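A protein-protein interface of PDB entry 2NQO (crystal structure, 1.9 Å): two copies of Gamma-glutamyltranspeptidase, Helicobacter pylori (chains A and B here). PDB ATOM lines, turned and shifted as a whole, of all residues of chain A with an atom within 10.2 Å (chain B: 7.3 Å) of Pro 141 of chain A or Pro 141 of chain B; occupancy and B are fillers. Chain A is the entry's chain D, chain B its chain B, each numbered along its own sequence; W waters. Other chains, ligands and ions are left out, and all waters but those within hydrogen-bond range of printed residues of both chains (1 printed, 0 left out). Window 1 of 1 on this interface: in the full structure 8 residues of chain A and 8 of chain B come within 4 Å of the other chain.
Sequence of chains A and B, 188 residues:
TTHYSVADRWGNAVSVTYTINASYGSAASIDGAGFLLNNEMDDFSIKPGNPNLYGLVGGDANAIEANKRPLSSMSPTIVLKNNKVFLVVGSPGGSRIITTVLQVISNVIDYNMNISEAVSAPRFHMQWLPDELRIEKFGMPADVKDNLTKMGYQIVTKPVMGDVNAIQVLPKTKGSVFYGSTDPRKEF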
ATOM      1  N   TYR A 111     -23.532 -11.968 -18.048  1.00  0.00           N
ATOM      2  CA  TYR A 111     -22.334 -11.703 -18.831  1.00  0.00           C
ATOM      3  C   TYR A 111     -22.553 -10.968 -20.151  1.00  0.00           C
ATOM      4  O   TYR A 111     -21.616 -10.770 -20.918  1.00  0.00           O
ATOM      5  CB  TYR A 111     -21.601 -13.036 -19.051  1.00  0.00           C
ATOM      6  CG  TYR A 111     -21.429 -13.807 -17.757  1.00  0.00           C
ATOM      7  CD1 TYR A 111     -20.900 -13.184 -16.624  1.00  0.00           C
ATOM      8  CD2 TYR A 111     -21.837 -15.141 -17.645  1.00  0.00           C
ATOM      9  CE1 TYR A 111     -20.787 -13.863 -15.412  1.00  0.00           C
ATOM     10  CE2 TYR A 111     -21.725 -15.833 -16.428  1.00  0.00           C
ATOM     11  CZ  TYR A 111     -21.200 -15.184 -15.320  1.00  0.00           C
ATOM     12  OH  TYR A 111     -21.074 -15.841 -14.122  1.00  0.00           O
ATOM     13  N   MET A 113     -23.875 -11.815 -23.000  1.00  0.00           N
ATOM     14  CA  MET A 113     -23.522 -12.511 -24.230  1.00  0.00           C
ATOM     15  C   MET A 113     -24.737 -12.404 -25.145  1.00  0.00           C
ATOM     16  O   MET A 113     -25.855 -12.232 -24.661  1.00  0.00           O
ATOM     17  CB  MET A 113     -23.253 -14.003 -23.970  1.00  0.00           C
ATOM     18  CG  MET A 113     -22.033 -14.330 -23.118  1.00  0.00           C
ATOM     19  SD  MET A 113     -21.726 -16.119 -23.118  1.00  0.00           S
ATOM     20  CE  MET A 113     -20.383 -16.257 -21.965  1.00  0.00           C
ATOM     21  N   PRO A 122     -19.502 -23.165 -22.832  1.00  0.00           N
ATOM     22  CA  PRO A 122     -19.428 -24.442 -22.107  1.00  0.00           C
ATOM     23  C   PRO A 122     -20.339 -24.425 -20.879  1.00  0.00           C
ATOM     24  O   PRO A 122     -20.536 -23.386 -20.276  1.00  0.00           O
ATOM     25  CB  PRO A 122     -17.955 -24.537 -21.728  1.00  0.00           C
ATOM     26  CG  PRO A 122     -17.273 -23.862 -22.881  1.00  0.00           C
ATOM     27  CD  PRO A 122     -18.150 -22.648 -23.125  1.00  0.00           C
ATOM     28  N   LEU A 133     -18.899 -32.390 -10.046  1.00  0.00           N
ATOM     29  CA  LEU A 133     -19.123 -31.213 -10.861  1.00  0.00           C
ATOM     30  C   LEU A 133     -18.860 -31.659 -12.294  1.00  0.00           C
ATOM     31  O   LEU A 133     -17.716 -31.851 -12.709  1.00  0.00           O
ATOM     32  CB  LEU A 133     -18.177 -30.076 -10.470  1.00  0.00           C
ATOM     33  CG  LEU A 133     -18.443 -28.785 -11.257  1.00  0.00           C
ATOM     34  CD1 LEU A 133     -19.848 -28.283 -10.964  1.00  0.00           C
ATOM     35  CD2 LEU A 133     -17.419 -27.733 -10.875  1.00  0.00           C
ATOM     36  N   ILE A 135     -18.597 -31.357 -16.241  1.00  0.00           N
ATOM     37  CA  ILE A 135     -18.207 -30.360 -17.231  1.00  0.00           C
ATOM     38  C   ILE A 135     -18.111 -30.990 -18.621  1.00  0.00           C
ATOM     39  O   ILE A 135     -18.292 -32.201 -18.782  1.00  0.00           O
ATOM     40  CB  ILE A 135     -16.832 -29.711 -16.897  1.00  0.00           C
ATOM     41  CG1 ILE A 135     -15.730 -30.769 -16.936  1.00  0.00           C
ATOM     42  CG2 ILE A 135     -16.890 -29.006 -15.545  1.00  0.00           C
ATOM     43  CD1 ILE A 135     -14.328 -30.195 -16.740  1.00  0.00           C
ATOM     44  N   GLU A 136     -17.815 -30.160 -19.618  1.00  0.00           N
ATOM     45  CA  GLU A 136     -17.701 -30.611 -21.000  1.00  0.00           C
ATOM     46  C   GLU A 136     -16.263 -30.487 -21.490  1.00  0.00           C
ATOM     47  O   GLU A 136     -15.488 -29.675 -20.986  1.00  0.00           O
ATOM     48  CB  GLU A 136     -18.622 -29.785 -21.905  1.00  0.00           C
ATOM     49  CG  GLU A 136     -20.073 -29.767 -21.454  1.00  0.00           C
ATOM     50  CD  GLU A 136     -20.944 -28.872 -22.319  1.00  0.00           C
ATOM     51  OE1 GLU A 136     -20.609 -27.677 -22.466  1.00  0.00           O
ATOM     52  OE2 GLU A 136     -21.967 -29.358 -22.845  1.00  0.00           O
ATOM     53  N   LYS A 137     -15.919 -31.291 -22.486  1.00  0.00           N
ATOM     54  CA  LYS A 137     -14.574 -31.284 -23.044  1.00  0.00           C
ATOM     55  C   LYS A 137     -14.205 -29.884 -23.534  1.00  0.00           C
ATOM     56  O   LYS A 137     -14.995 -29.226 -24.208  1.00  0.00           O
ATOM     57  CB  LYS A 137     -14.499 -32.286 -24.198  1.00  0.00           C
ATOM     58  CG  LYS A 137     -13.094 -32.653 -24.623  1.00  0.00           C
ATOM     59  CD  LYS A 137     -13.139 -33.628 -25.786  1.00  0.00           C
ATOM     60  CE  LYS A 137     -11.741 -34.036 -26.220  1.00  0.00           C
ATOM     61  NZ  LYS A 137     -11.784 -34.849 -27.469  1.00  0.00           N
ATOM     62  N   PHE A 138     -13.003 -29.435 -23.186  1.00  0.00           N
ATOM     63  CA  PHE A 138     -12.518 -28.109 -23.579  1.00  0.00           C
ATOM     64  C   PHE A 138     -13.319 -27.000 -22.913  1.00  0.00           C
ATOM     65  O   PHE A 138     -13.129 -25.825 -23.214  1.00  0.00           O
ATOM     66  CB  PHE A 138     -12.611 -27.919 -25.101  1.00  0.00           C
ATOM     67  CG  PHE A 138     -11.942 -29.000 -25.897  1.00  0.00           C
ATOM     68  CD1 PHE A 138     -10.619 -29.342 -25.659  1.00  0.00           C
ATOM     69  CD2 PHE A 138     -12.646 -29.685 -26.884  1.00  0.00           C
ATOM     70  CE1 PHE A 138     -10.002 -30.357 -26.392  1.00  0.00           C
ATOM     71  CE2 PHE A 138     -12.037 -30.701 -27.623  1.00  0.00           C
ATOM     72  CZ  PHE A 138     -10.714 -31.036 -27.376  1.00  0.00           C
ATOM     73  N   GLY A 139     -14.209 -27.369 -21.998  1.00  0.00           N
ATOM     74  CA  GLY A 139     -15.043 -26.372 -21.351  1.00  0.00           C
ATOM     75  C   GLY A 139     -14.474 -25.646 -20.148  1.00  0.00           C
ATOM     76  O   GLY A 139     -14.929 -24.555 -19.808  1.00  0.00           O
ATOM     77  N   MET A 140     -13.478 -26.230 -19.502  1.00  0.00           N
ATOM     78  CA  MET A 140     -12.909 -25.592 -18.324  1.00  0.00           C
ATOM     79  C   MET A 140     -11.392 -25.751 -18.282  1.00  0.00           C
ATOM     80  O   MET A 140     -10.873 -26.868 -18.257  1.00  0.00           O
ATOM     81  CB  MET A 140     -13.553 -26.197 -17.079  1.00  0.00           C
ATOM     82  CG  MET A 140     -13.147 -25.576 -15.772  1.00  0.00           C
ATOM     83  SD  MET A 140     -13.953 -26.473 -14.436  1.00  0.00           S
ATOM     84  CE  MET A 140     -15.584 -25.776 -14.529  1.00  0.00           C
ATOM     85  N   PRO A 141     -10.660 -24.628 -18.287  1.00  0.00           N
ATOM     86  CA  PRO A 141      -9.198 -24.693 -18.250  1.00  0.00           C
ATOM     87  C   PRO A 141      -8.638 -25.188 -16.917  1.00  0.00           C
ATOM     88  O   PRO A 141      -9.301 -25.128 -15.880  1.00  0.00           O
ATOM     89  CB  PRO A 141      -8.779 -23.258 -18.574  1.00  0.00           C
ATOM     90  CG  PRO A 141      -9.878 -22.446 -17.993  1.00  0.00           C
ATOM     91  CD  PRO A 141     -11.122 -23.231 -18.395  1.00  0.00           C
ATOM     92  N   ALA A 142      -7.401 -25.671 -16.963  1.00  0.00           N
ATOM     93  CA  ALA A 142      -6.715 -26.197 -15.793  1.00  0.00           C
ATOM     94  C   ALA A 142      -6.788 -25.281 -14.576  1.00  0.00           C
ATOM     95  O   ALA A 142      -7.087 -25.732 -13.471  1.00  0.00           O
ATOM     96  CB  ALA A 142      -5.261 -26.484 -16.144  1.00  0.00           C
ATOM     97  N   ASP A 143      -6.524 -23.994 -14.776  1.00  0.00           N
ATOM     98  CA  ASP A 143      -6.545 -23.032 -13.679  1.00  0.00           C
ATOM     99  C   ASP A 143      -7.859 -23.017 -12.904  1.00  0.00           C
ATOM    100  O   ASP A 143      -7.855 -22.955 -11.669  1.00  0.00           O
ATOM    101  CB  ASP A 143      -6.262 -21.627 -14.209  1.00  0.00           C
ATOM    102  CG  ASP A 143      -4.897 -21.519 -14.851  1.00  0.00           C
ATOM    103  OD1 ASP A 143      -4.617 -22.310 -15.775  1.00  0.00           O
ATOM    104  OD2 ASP A 143      -4.107 -20.643 -14.430  1.00  0.00           O
ATOM    105  N   VAL A 144      -8.972 -23.053 -13.637  1.00  0.00           N
ATOM    106  CA  VAL A 144     -10.302 -23.049 -13.044  1.00  0.00           C
ATOM    107  C   VAL A 144     -10.579 -24.393 -12.388  1.00  0.00           C
ATOM    108  O   VAL A 144     -11.064 -24.453 -11.257  1.00  0.00           O
ATOM    109  CB  VAL A 144     -11.398 -22.775 -14.111  1.00  0.00           C
ATOM    110  CG1 VAL A 144     -12.787 -22.842 -13.466  1.00  0.00           C
ATOM    111  CG2 VAL A 144     -11.183 -21.402 -14.746  1.00  0.00           C
ATOM    112  N   LYS A 145     -10.271 -25.473 -13.099  1.00  0.00           N
ATOM    113  CA  LYS A 145     -10.481 -26.802 -12.555  1.00  0.00           C
ATOM    114  C   LYS A 145      -9.691 -26.962 -11.265  1.00  0.00           C
ATOM    115  O   LYS A 145     -10.214 -27.475 -10.274  1.00  0.00           O
ATOM    116  CB  LYS A 145     -10.064 -27.880 -13.565  1.00  0.00           C
ATOM    117  CG  LYS A 145     -10.972 -27.955 -14.782  1.00  0.00           C
ATOM    118  CD  LYS A 145     -10.732 -29.204 -15.630  1.00  0.00           C
ATOM    119  CE  LYS A 145      -9.395 -29.177 -16.339  1.00  0.00           C
ATOM    120  NZ  LYS A 145      -9.273 -30.327 -17.279  1.00  0.00           N
ATOM    121  N   ASP A 146      -8.437 -26.515 -11.261  1.00  0.00           N
ATOM    122  CA  ASP A 146      -7.616 -26.644 -10.058  1.00  0.00           C
ATOM    123  C   ASP A 146      -8.218 -25.914  -8.855  1.00  0.00           C
ATOM    124  O   ASP A 146      -8.261 -26.468  -7.754  1.00  0.00           O
ATOM    125  CB  ASP A 146      -6.184 -26.137 -10.302  1.00  0.00           C
ATOM    126  CG  ASP A 146      -5.374 -27.060 -11.204  1.00  0.00           C
ATOM    127  OD1 ASP A 146      -5.768 -28.233 -11.392  1.00  0.00           O
ATOM    128  OD2 ASP A 146      -4.328 -26.609 -11.716  1.00  0.00           O
ATOM    129  N   ASN A 147      -8.677 -24.678  -9.058  1.00  0.00           N
ATOM    130  CA  ASN A 147      -9.269 -23.913  -7.969  1.00  0.00           C
ATOM    131  C   ASN A 147     -10.557 -24.551  -7.454  1.00  0.00           C
ATOM    132  O   ASN A 147     -10.788 -24.604  -6.244  1.00  0.00           O
ATOM    133  CB  ASN A 147      -9.529 -22.460  -8.394  1.00  0.00           C
ATOM    134  CG  ASN A 147      -8.250 -21.630  -8.446  1.00  0.00           C
ATOM    135  OD1 ASN A 147      -7.329 -21.848  -7.663  1.00  0.00           O
ATOM    136  ND2 ASN A 147      -8.198 -20.665  -9.355  1.00  0.00           N
ATOM    137  N   LEU A 148     -11.391 -25.045  -8.366  1.00  0.00           N
ATOM    138  CA  LEU A 148     -12.642 -25.691  -7.973  1.00  0.00           C
ATOM    139  C   LEU A 148     -12.358 -26.996  -7.222  1.00  0.00           C
ATOM    140  O   LEU A 148     -13.026 -27.319  -6.229  1.00  0.00           O
ATOM    141  CB  LEU A 148     -13.496 -25.973  -9.211  1.00  0.00           C
ATOM    142  CG  LEU A 148     -14.058 -24.737  -9.921  1.00  0.00           C
ATOM    143  CD1 LEU A 148     -14.782 -25.151 -11.198  1.00  0.00           C
ATOM    144  CD2 LEU A 148     -15.003 -23.995  -8.972  1.00  0.00           C
ATOM    145  N   THR A 149     -11.364 -27.741  -7.697  1.00  0.00           N
ATOM    146  CA  THR A 149     -10.975 -28.993  -7.055  1.00  0.00           C
ATOM    147  C   THR A 149     -10.515 -28.710  -5.624  1.00  0.00           C
ATOM    148  O   THR A 149     -10.861 -29.444  -4.693  1.00  0.00           O
ATOM    149  CB  THR A 149      -9.830 -29.694  -7.833  1.00  0.00           C
ATOM    150  OG1 THR A 149     -10.332 -30.182  -9.086  1.00  0.00           O
ATOM    151  CG2 THR A 149      -9.271 -30.870  -7.034  1.00  0.00           C
ATOM    152  N   ILE A 155     -14.362 -32.996 -10.102  1.00  0.00           N
ATOM    153  CA  ILE A 155     -14.667 -32.682 -11.488  1.00  0.00           C
ATOM    154  C   ILE A 155     -14.607 -33.895 -12.403  1.00  0.00           C
ATOM    155  O   ILE A 155     -13.689 -34.706 -12.310  1.00  0.00           O
ATOM    156  CB  ILE A 155     -13.695 -31.608 -12.016  1.00  0.00           C
ATOM    157  CG1 ILE A 155     -13.813 -30.349 -11.156  1.00  0.00           C
ATOM    158  CG2 ILE A 155     -13.996 -31.304 -13.480  1.00  0.00           C
ATOM    159  CD1 ILE A 155     -12.794 -29.267 -11.482  1.00  0.00           C
ATOM    160  N   THR A 157     -15.442 -35.026 -16.643  1.00  0.00           N
ATOM    161  CA  THR A 157     -15.790 -34.599 -17.987  1.00  0.00           C
ATOM    162  C   THR A 157     -16.667 -35.664 -18.619  1.00  0.00           C
ATOM    163  O   THR A 157     -16.293 -36.837 -18.672  1.00  0.00           O
ATOM    164  CB  THR A 157     -14.538 -34.399 -18.848  1.00  0.00           C
ATOM    165  OG1 THR A 157     -13.695 -33.420 -18.231  1.00  0.00           O
ATOM    166  CG2 THR A 157     -14.918 -33.933 -20.241  1.00  0.00           C
ATOM    167  N   ILE B 135      -6.051 -10.650 -25.681  1.00  0.00           N
ATOM    168  CA  ILE B 135      -7.031 -11.731 -25.625  1.00  0.00           C
ATOM    169  C   ILE B 135      -8.362 -11.284 -26.218  1.00  0.00           C
ATOM    170  O   ILE B 135      -8.540 -10.109 -26.554  1.00  0.00           O
ATOM    171  CB  ILE B 135      -7.268 -12.234 -24.175  1.00  0.00           C
ATOM    172  CG1 ILE B 135      -7.798 -11.110 -23.286  1.00  0.00           C
ATOM    173  CG2 ILE B 135      -5.976 -12.776 -23.605  1.00  0.00           C
ATOM    174  CD1 ILE B 135      -8.414 -11.615 -21.977  1.00  0.00           C
ATOM    175  N   PHE B 138     -14.638 -12.904 -23.667  1.00  0.00           N
ATOM    176  CA  PHE B 138     -15.087 -14.222 -23.200  1.00  0.00           C
ATOM    177  C   PHE B 138     -14.060 -15.322 -23.451  1.00  0.00           C
ATOM    178  O   PHE B 138     -14.338 -16.502 -23.227  1.00  0.00           O
ATOM    179  CB  PHE B 138     -16.410 -14.627 -23.873  1.00  0.00           C
ATOM    180  CG  PHE B 138     -17.539 -13.660 -23.640  1.00  0.00           C
ATOM    181  CD1 PHE B 138     -17.903 -13.288 -22.349  1.00  0.00           C
ATOM    182  CD2 PHE B 138     -18.241 -13.119 -24.720  1.00  0.00           C
ATOM    183  CE1 PHE B 138     -18.949 -12.385 -22.132  1.00  0.00           C
ATOM    184  CE2 PHE B 138     -19.287 -12.218 -24.516  1.00  0.00           C
ATOM    185  CZ  PHE B 138     -19.643 -11.849 -23.219  1.00  0.00           C
ATOM    186  N   GLY B 139     -12.869 -14.939 -23.898  1.00  0.00           N
ATOM    187  CA  GLY B 139     -11.856 -15.930 -24.207  1.00  0.00           C
ATOM    188  C   GLY B 139     -11.005 -16.476 -23.079  1.00  0.00           C
ATOM    189  O   GLY B 139     -10.389 -17.528 -23.224  1.00  0.00           O
ATOM    190  N   MET B 140     -10.973 -15.782 -21.950  1.00  0.00           N
ATOM    191  CA  MET B 140     -10.147 -16.214 -20.830  1.00  0.00           C
ATOM    192  C   MET B 140     -10.830 -15.925 -19.493  1.00  0.00           C
ATOM    193  O   MET B 140     -11.164 -14.779 -19.198  1.00  0.00           O
ATOM    194  CB  MET B 140      -8.803 -15.483 -20.913  1.00  0.00           C
ATOM    195  CG  MET B 140      -7.780 -15.874 -19.872  1.00  0.00           C
ATOM    196  SD  MET B 140      -6.276 -14.875 -20.066  1.00  0.00           S
ATOM    197  CE  MET B 140      -5.537 -15.689 -21.464  1.00  0.00           C
ATOM    198  N   PRO B 141     -11.063 -16.966 -18.674  1.00  0.00           N
ATOM    199  CA  PRO B 141     -11.712 -16.791 -17.371  1.00  0.00           C
ATOM    200  C   PRO B 141     -10.815 -16.132 -16.330  1.00  0.00           C
ATOM    201  O   PRO B 141      -9.591 -16.208 -16.417  1.00  0.00           O
ATOM    202  CB  PRO B 141     -12.089 -18.217 -16.982  1.00  0.00           C
ATOM    203  CG  PRO B 141     -10.981 -19.021 -17.589  1.00  0.00           C
ATOM    204  CD  PRO B 141     -10.877 -18.399 -18.968  1.00  0.00           C
ATOM    205  N   ALA B 142     -11.447 -15.506 -15.341  1.00  0.00           N
ATOM    206  CA  ALA B 142     -10.753 -14.814 -14.261  1.00  0.00           C
ATOM    207  C   ALA B 142      -9.547 -15.560 -13.680  1.00  0.00           C
ATOM    208  O   ALA B 142      -8.472 -14.983 -13.531  1.00  0.00           O
ATOM    209  CB  ALA B 142     -11.748 -14.489 -13.147  1.00  0.00           C
ATOM    210  N   ASP B 143      -9.730 -16.837 -13.351  1.00  0.00           N
ATOM    211  CA  ASP B 143      -8.665 -17.650 -12.769  1.00  0.00           C
ATOM    212  C   ASP B 143      -7.394 -17.655 -13.605  1.00  0.00           C
ATOM    213  O   ASP B 143      -6.290 -17.580 -13.065  1.00  0.00           O
ATOM    214  CB  ASP B 143      -9.137 -19.095 -12.581  1.00  0.00           C
ATOM    215  CG  ASP B 143     -10.352 -19.202 -11.672  1.00  0.00           C
ATOM    216  OD1 ASP B 143     -11.343 -18.482 -11.914  1.00  0.00           O
ATOM    217  OD2 ASP B 143     -10.315 -20.008 -10.719  1.00  0.00           O
ATOM    218  N   VAL B 144      -7.561 -17.764 -14.920  1.00  0.00           N
ATOM    219  CA  VAL B 144      -6.439 -17.797 -15.850  1.00  0.00           C
ATOM    220  C   VAL B 144      -5.779 -16.427 -15.944  1.00  0.00           C
ATOM    221  O   VAL B 144      -4.557 -16.314 -15.865  1.00  0.00           O
ATOM    222  CB  VAL B 144      -6.904 -18.229 -17.261  1.00  0.00           C
ATOM    223  CG1 VAL B 144      -5.732 -18.204 -18.243  1.00  0.00           C
ATOM    224  CG2 VAL B 144      -7.517 -19.618 -17.197  1.00  0.00           C
ATOM    225  N   LYS B 145      -6.592 -15.389 -16.117  1.00  0.00           N
ATOM    226  CA  LYS B 145      -6.066 -14.036 -16.209  1.00  0.00           C
ATOM    227  C   LYS B 145      -5.295 -13.671 -14.938  1.00  0.00           C
ATOM    228  O   LYS B 145      -4.214 -13.075 -15.007  1.00  0.00           O
ATOM    229  CB  LYS B 145      -7.203 -13.039 -16.453  1.00  0.00           C
ATOM    230  CG  LYS B 145      -7.945 -13.297 -17.759  1.00  0.00           C
ATOM    231  CD  LYS B 145      -8.783 -12.118 -18.229  1.00  0.00           C
ATOM    232  CE  LYS B 145     -10.033 -11.930 -17.399  1.00  0.00           C
ATOM    233  NZ  LYS B 145     -10.908 -10.893 -18.019  1.00  0.00           N
ATOM    234  N   ASP B 146      -5.839 -14.037 -13.782  1.00  0.00           N
ATOM    235  CA  ASP B 146      -5.172 -13.738 -12.520  1.00  0.00           C
ATOM    236  C   ASP B 146      -3.787 -14.370 -12.459  1.00  0.00           C
ATOM    237  O   ASP B 146      -2.816 -13.721 -12.075  1.00  0.00           O
ATOM    238  CB  ASP B 146      -5.998 -14.234 -11.329  1.00  0.00           C
ATOM    239  CG  ASP B 146      -7.276 -13.443 -11.134  1.00  0.00           C
ATOM    240  OD1 ASP B 146      -7.378 -12.333 -11.699  1.00  0.00           O
ATOM    241  OD2 ASP B 146      -8.172 -13.927 -10.406  1.00  0.00           O
ATOM    242  N   ASN B 147      -3.687 -15.636 -12.841  1.00  0.00           N
ATOM    243  CA  ASN B 147      -2.400 -16.305 -12.795  1.00  0.00           C
ATOM    244  C   ASN B 147      -1.396 -15.746 -13.800  1.00  0.00           C
ATOM    245  O   ASN B 147      -0.197 -15.685 -13.515  1.00  0.00           O
ATOM    246  CB  ASN B 147      -2.581 -17.812 -12.972  1.00  0.00           C
ATOM    247  CG  ASN B 147      -3.226 -18.458 -11.755  1.00  0.00           C
ATOM    248  OD1 ASN B 147      -3.128 -17.937 -10.643  1.00  0.00           O
ATOM    249  ND2 ASN B 147      -3.876 -19.598 -11.955  1.00  0.00           N
ATOM    250  N   ILE B 155      -2.508  -8.031 -19.512  1.00  0.00           N
ATOM    251  CA  ILE B 155      -3.623  -8.509 -20.329  1.00  0.00           C
ATOM    252  C   ILE B 155      -4.547  -7.414 -20.861  1.00  0.00           C
ATOM    253  O   ILE B 155      -4.988  -6.547 -20.112  1.00  0.00           O
ATOM    254  CB  ILE B 155      -4.462  -9.531 -19.519  1.00  0.00           C
ATOM    255  CG1 ILE B 155      -3.569 -10.703 -19.099  1.00  0.00           C
ATOM    256  CG2 ILE B 155      -5.648 -10.016 -20.341  1.00  0.00           C
ATOM    257  CD1 ILE B 155      -4.199 -11.652 -18.088  1.00  0.00           C
HETATM  258  O   HOH W   1      -6.474 -18.278 -10.076  1.00  0.00           O
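Pro 141 of chain A touches just these residues of chain B: Pro 141 and Val 144. Pro 141 of chain B touches just these residues of chain A: Pro 141 (3.6 Å) and Val 144 (3.7 Å). Val 144 of chain B touches just these residues of chain A: Pro 141 (3.8 Å) and Asp 143 (3.8 Å). Of the printed residues of chain A, Asn 147 of chain B touches Asp 143. Of the printed residues of chain A, Asp 143 of chain B touches Asp 143 (3.95 Å), Val 144 (3.8 Å) and Asn 147 (2.6 Å). Met 140 of chain B touches none of the printed residues of chain A. The nearest residue of chain A that does not touch Pro 141 of chain B is Asp 143 of chain A (6.4 Å). The nearest printed residue of chain B that does not touch Asn 147 of chain A is Asn 147 of chain B (5.2 Å).
The side-chain amide nitrogen (ND2) of Asn 147 of chain A sits at hydrogen-bond distance from the backbone carbonyl oxygen (O) of Asp 143 of chain A. The backbone carbonyl oxygen (O) of Asp 143 of chain B lies within hydrogen-bond range of the side-chain amide nitrogen (ND2) of Asn 147 of chain B (3.3 Å).
The side-chain carboxylate (OD2) of Asp 143 of chain A sits at hydrogen-bond distance from the side-chain amide nitrogen (ND2) of Asn 147 of chain B (2.7 Å). The side-chain carboxylate (OD2) of Asp 143 of chain B is in hydrogen-bond range of the side-chain amide nitrogen (ND2) of Asn 147 of chain A, at 2.6 Å.
Pro 141 of chain A touches its own counterpart, Pro 141 of chain B. Pro 141 of chain A touches Val 144 of chain B, and with the chains exchanged Val 144 of chain A touches Pro 141 of chain B. Asp 143 of chain B touches its own counterpart, Asp 143 of chain A. Asp 143 of chain A touches Val 144 of chain B, and with the chains exchanged Val 144 of chain A touches Asp 143 of chain B.
Of the 21 printed residues of chain A, 6 touch a printed residue of chain B. Printed residues of chain A that touch a printed residue of chain B: Tyr 111, Met 113, Pro 141, Asp 143, Val 144 and Asn 147. Hydrophobic or aromatic side chains of chain A within 4 Å of the printed part of chain B: Met 113, Pro 141 and Val 144. Of the 12 printed residues of chain B, 5 touch a printed residue of chain A. Printed residues of chain B that touch a printed residue of chain A: Phe 138, Pro 141, Asp 143, Val 144 and Asn 147. Among the printed residues, 10 pairs touch across the chains. Among the printed residues, no Asp or Glu carboxylate lies within 4 Å of a Lys or Arg side-chain nitrogen of the other chain.
Tyr 111 of chain A touches Phe 138 of chain B. Met 113 of chain A touches Phe 138 of chain B (CG to CZ, 3.4 Å). Pro 141 of chain B touches Pro 141 of chain A. Pro 141 of chain A touches Val 144 of chain B (CG to CG2, 3.8 Å). OD2 of Asp 143 of chain B touches O of Asp 143 of chain A, at 3.95 Å. CB of Asp 143 of chain A touches CG2 of Val 144 of chain B, 3.8 Å away. Val 144 of chain A touches Pro 141 of chain B (CG2 to CG, 3.7 Å). CG2 of Val 144 of chain A touches CB of Asp 143 of chain B (3.8 Å).
Water W1 lies within hydrogen-bond range of the side-chain amide nitrogen of Asn 147 of chain A (3.0 Å), the backbone carbonyl oxygen of Asp 143 of chain B (3.1 Å) and the side-chain amide oxygen of Asn 147 of chain B (3.4 Å).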
